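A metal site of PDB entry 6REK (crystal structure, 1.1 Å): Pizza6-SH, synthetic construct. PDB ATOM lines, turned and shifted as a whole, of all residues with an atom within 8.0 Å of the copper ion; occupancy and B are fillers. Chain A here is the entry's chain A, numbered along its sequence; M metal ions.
The copper ion is bound by a ring nitrogen (NE2) of His 119, a ring nitrogen (ND1) of His 161 and a ring nitrogen (NE2) of His 146.
Thr 144 touches the copper ion (CB to CU, 3.8 Å). Of the 16 residues printed, 4 come within 4 Å of the copper ion.
The backbone carbonyl oxygen of Thr 102 sits at hydrogen-bond distance from the backbone NH of His 119 (3.0 Å). The backbone carbonyl oxygen (O) of Thr 144 sits at hydrogen-bond distance from the backbone NH (N) of His 161. A ring nitrogen (NE2) of His 161 sits at hydrogen-bond distance from the side-chain hydroxyl (OG1) of Thr 186. The side-chain hydroxyl (OG) of Ser 104 lies within hydrogen-bond range of the backbone carbonyl oxygen (O) of His 146 (2.9 Å). The backbone NH of His 146 sits at hydrogen-bond distance from the backbone carbonyl oxygen of Thr 159, at 3.0 Å. The side-chain hydroxyl of Thr 144 sits at hydrogen-bond distance from the backbone NH of Gly 162 (2.9 Å). OD1 of Asn 143 is in hydrogen-bond range of OG1 of Thr 144 (2.7 Å). N of Thr 144 lies within hydrogen-bond range of OD1 of Asn 122, 2.8 Å away.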
ATOM      1  N   THR A 102     -26.553   6.741 -24.636  1.00  0.00           N
ATOM      2  CA  THR A 102     -27.406   5.548 -24.615  1.00  0.00           C
ATOM      3  C   THR A 102     -27.446   4.909 -23.230  1.00  0.00           C
ATOM      4  O   THR A 102     -27.000   3.761 -23.034  1.00  0.00           O
ATOM      5  CB  THR A 102     -27.025   4.525 -25.687  1.00  0.00           C
ATOM      6  OG1 THR A 102     -26.784   5.194 -26.918  1.00  0.00           O
ATOM      7  CG2 THR A 102     -28.169   3.537 -25.923  1.00  0.00           C
ATOM      8  N   SER A 104     -28.880   2.613 -20.830  1.00  0.00           N
ATOM      9  CA  SER A 104     -29.585   1.414 -21.310  1.00  0.00           C
ATOM     10  C   SER A 104     -30.312   0.634 -20.232  1.00  0.00           C
ATOM     11  O   SER A 104     -31.245  -0.113 -20.530  1.00  0.00           O
ATOM     12  CB  SER A 104     -28.601   0.466 -22.029  1.00  0.00           C
ATOM     13  OG  SER A 104     -27.519   0.064 -21.198  1.00  0.00           O
ATOM     14  N   HIS A 119     -24.330   2.515 -22.379  1.00  0.00           N
ATOM     15  CA  HIS A 119     -24.000   1.560 -23.440  1.00  0.00           C
ATOM     16  C   HIS A 119     -22.961   2.124 -24.393  1.00  0.00           C
ATOM     17  O   HIS A 119     -21.992   1.448 -24.761  1.00  0.00           O
ATOM     18  CB  HIS A 119     -25.312   1.178 -24.176  1.00  0.00           C
ATOM     19  CG  HIS A 119     -25.164   0.248 -25.340  1.00  0.00           C
ATOM     20  ND1 HIS A 119     -24.970   0.677 -26.637  1.00  0.00           N
ATOM     21  CD2 HIS A 119     -25.253  -1.122 -25.419  1.00  0.00           C
ATOM     22  CE1 HIS A 119     -24.952  -0.370 -27.456  1.00  0.00           C
ATOM     23  NE2 HIS A 119     -25.105  -1.479 -26.743  1.00  0.00           N
ATOM     24  N   GLY A 120     -23.154   3.374 -24.818  1.00  0.00           N
ATOM     25  CA  GLY A 120     -22.280   3.976 -25.807  1.00  0.00           C
ATOM     26  C   GLY A 120     -20.927   4.370 -25.292  1.00  0.00           C
ATOM     27  O   GLY A 120     -20.057   4.682 -26.105  1.00  0.00           O
ATOM     28  N   ASN A 122     -19.338   2.312 -22.946  1.00  0.00           N
ATOM     29  CA  ASN A 122     -18.703   1.096 -22.470  1.00  0.00           C
ATOM     30  C   ASN A 122     -18.442   1.130 -20.968  1.00  0.00           C
ATOM     31  O   ASN A 122     -17.395   0.674 -20.507  1.00  0.00           O
ATOM     32  CB  ASN A 122     -17.409   0.800 -23.252  1.00  0.00           C
ATOM     33  CG  ASN A 122     -17.709   0.566 -24.696  1.00  0.00           C
ATOM     34  OD1 ASN A 122     -18.678  -0.095 -25.039  1.00  0.00           O
ATOM     35  ND2 ASN A 122     -16.900   1.148 -25.566  1.00  0.00           N
ATOM     36  N   ASN A 143     -17.712  -3.934 -22.467  1.00  0.00           N
ATOM     37  CA  ASN A 143     -18.167  -3.371 -23.717  1.00  0.00           C
ATOM     38  C   ASN A 143     -19.723  -3.346 -23.758  1.00  0.00           C
ATOM     39  O   ASN A 143     -20.377  -4.253 -23.222  1.00  0.00           O
ATOM     40  CB  ASN A 143     -17.624  -4.203 -24.853  1.00  0.00           C
ATOM     41  CG  ASN A 143     -17.773  -3.513 -26.192  1.00  0.00           C
ATOM     42  OD1 ASN A 143     -18.706  -3.760 -26.953  1.00  0.00           O
ATOM     43  ND2 ASN A 143     -16.856  -2.552 -26.457  1.00  0.00           N
ATOM     44  N   THR A 144     -20.256  -2.275 -24.288  1.00  0.00           N
ATOM     45  CA  THR A 144     -21.649  -2.156 -24.581  1.00  0.00           C
ATOM     46  C   THR A 144     -22.547  -2.833 -23.558  1.00  0.00           C
ATOM     47  O   THR A 144     -23.278  -3.778 -23.875  1.00  0.00           O
ATOM     48  CB  THR A 144     -21.931  -2.590 -26.025  1.00  0.00           C
ATOM     49  OG1 THR A 144     -21.327  -3.854 -26.334  1.00  0.00           O
ATOM     50  CG2 THR A 144     -21.395  -1.577 -26.997  1.00  0.00           C
ATOM     51  N   PRO A 145     -22.596  -2.293 -22.358  1.00  0.00           N
ATOM     52  CA  PRO A 145     -23.471  -2.869 -21.331  1.00  0.00           C
ATOM     53  C   PRO A 145     -24.934  -2.571 -21.637  1.00  0.00           C
ATOM     54  O   PRO A 145     -25.295  -1.447 -22.040  1.00  0.00           O
ATOM     55  CB  PRO A 145     -23.044  -2.175 -20.046  1.00  0.00           C
ATOM     56  CG  PRO A 145     -22.470  -0.825 -20.519  1.00  0.00           C
ATOM     57  CD  PRO A 145     -21.752  -1.220 -21.829  1.00  0.00           C
ATOM     58  N   HIS A 146     -25.791  -3.558 -21.444  1.00  0.00           N
ATOM     59  CA  HIS A 146     -27.231  -3.335 -21.594  1.00  0.00           C
ATOM     60  C   HIS A 146     -27.893  -3.255 -20.228  1.00  0.00           C
ATOM     61  O   HIS A 146     -28.342  -2.246 -19.744  1.00  0.00           O
ATOM     62  CB  HIS A 146     -27.872  -4.450 -22.455  1.00  0.00           C
ATOM     63  CG  HIS A 146     -27.639  -4.280 -23.922  1.00  0.00           C
ATOM     64  ND1 HIS A 146     -28.643  -4.006 -24.820  1.00  0.00           N
ATOM     65  CD2 HIS A 146     -26.483  -4.229 -24.636  1.00  0.00           C
ATOM     66  CE1 HIS A 146     -28.129  -3.872 -26.032  1.00  0.00           C
ATOM     67  NE2 HIS A 146     -26.815  -3.997 -25.942  1.00  0.00           N
ATOM     68  N   THR A 159     -24.968  -7.001 -17.983  1.00  0.00           N
ATOM     69  CA  THR A 159     -24.807  -7.737 -19.220  1.00  0.00           C
ATOM     70  C   THR A 159     -23.909  -6.955 -20.162  1.00  0.00           C
ATOM     71  O   THR A 159     -24.030  -5.720 -20.298  1.00  0.00           O
ATOM     72  CB  THR A 159     -26.154  -8.027 -19.899  1.00  0.00           C
ATOM     73  OG1 THR A 159     -26.767  -6.787 -20.240  1.00  0.00           O
ATOM     74  CG2 THR A 159     -27.088  -8.812 -19.002  1.00  0.00           C
ATOM     75  N   ASP A 160     -23.063  -7.661 -20.894  1.00  0.00           N
ATOM     76  CA  ASP A 160     -22.115  -7.087 -21.861  1.00  0.00           C
ATOM     77  C   ASP A 160     -22.453  -7.639 -23.235  1.00  0.00           C
ATOM     78  O   ASP A 160     -22.325  -8.846 -23.490  1.00  0.00           O
ATOM     79  CB  ASP A 160     -20.685  -7.454 -21.422  1.00  0.00           C
ATOM     80  CG  ASP A 160     -19.618  -6.953 -22.357  1.00  0.00           C
ATOM     81  OD1 ASP A 160     -18.480  -6.658 -21.880  1.00  0.00           O
ATOM     82  OD2 ASP A 160     -19.832  -6.918 -23.562  1.00  0.00           O
ATOM     83  N   HIS A 161     -22.933  -6.753 -24.124  1.00  0.00           N
ATOM     84  CA  HIS A 161     -23.310  -7.167 -25.467  1.00  0.00           C
ATOM     85  C   HIS A 161     -22.090  -7.594 -26.270  1.00  0.00           C
ATOM     86  O   HIS A 161     -22.056  -8.697 -26.838  1.00  0.00           O
ATOM     87  CB  HIS A 161     -24.047  -5.983 -26.099  1.00  0.00           C
ATOM     88  CG  HIS A 161     -24.507  -6.188 -27.494  1.00  0.00           C
ATOM     89  ND1 HIS A 161     -25.122  -5.169 -28.179  1.00  0.00           N
ATOM     90  CD2 HIS A 161     -24.453  -7.237 -28.346  1.00  0.00           C
ATOM     91  CE1 HIS A 161     -25.457  -5.579 -29.388  1.00  0.00           C
ATOM     92  NE2 HIS A 161     -25.059  -6.835 -29.523  1.00  0.00           N
ATOM     93  N   GLY A 162     -21.083  -6.722 -26.364  1.00  0.00           N
ATOM     94  CA  GLY A 162     -19.942  -6.983 -27.241  1.00  0.00           C
ATOM     95  C   GLY A 162     -19.204  -8.259 -26.919  1.00  0.00           C
ATOM     96  O   GLY A 162     -18.693  -8.916 -27.828  1.00  0.00           O
ATOM     97  N   THR A 186     -25.934 -11.637 -27.420  1.00  0.00           N
ATOM     98  CA  THR A 186     -26.605 -10.371 -27.106  1.00  0.00           C
ATOM     99  C   THR A 186     -27.433 -10.499 -25.824  1.00  0.00           C
ATOM    100  O   THR A 186     -28.662 -10.314 -25.840  1.00  0.00           O
ATOM    101  CB  THR A 186     -27.460  -9.846 -28.278  1.00  0.00           C
ATOM    102  OG1 THR A 186     -26.667  -9.926 -29.465  1.00  0.00           O
ATOM    103  CG2 THR A 186     -27.883  -8.411 -28.058  1.00  0.00           C
ATOM    104  N   PRO A 187     -26.814 -10.757 -24.687  1.00  0.00           N
ATOM    105  CA  PRO A 187     -27.553 -10.678 -23.423  1.00  0.00           C
ATOM    106  C   PRO A 187     -27.998  -9.243 -23.227  1.00  0.00           C
ATOM    107  O   PRO A 187     -27.217  -8.313 -23.365  1.00  0.00           O
ATOM    108  CB  PRO A 187     -26.516 -11.097 -22.364  1.00  0.00           C
ATOM    109  CG  PRO A 187     -25.170 -10.706 -23.009  1.00  0.00           C
ATOM    110  CD  PRO A 187     -25.364 -10.973 -24.480  1.00  0.00           C
ATOM    111  N   SER A 188     -29.262  -9.089 -22.941  1.00  0.00           N
ATOM    112  CA  SER A 188     -29.849  -7.780 -22.810  1.00  0.00           C
ATOM    113  C   SER A 188     -30.168  -7.509 -21.344  1.00  0.00           C
ATOM    114  O   SER A 188     -29.447  -6.844 -20.600  1.00  0.00           O
ATOM    115  CB  SER A 188     -31.060  -7.715 -23.750  1.00  0.00           C
ATOM    116  OG  SER A 188     -31.492  -6.410 -23.855  1.00  0.00           O
HETATM  117 CU    CU M   1     -25.388  -3.320 -27.459  1.00  0.00          CU
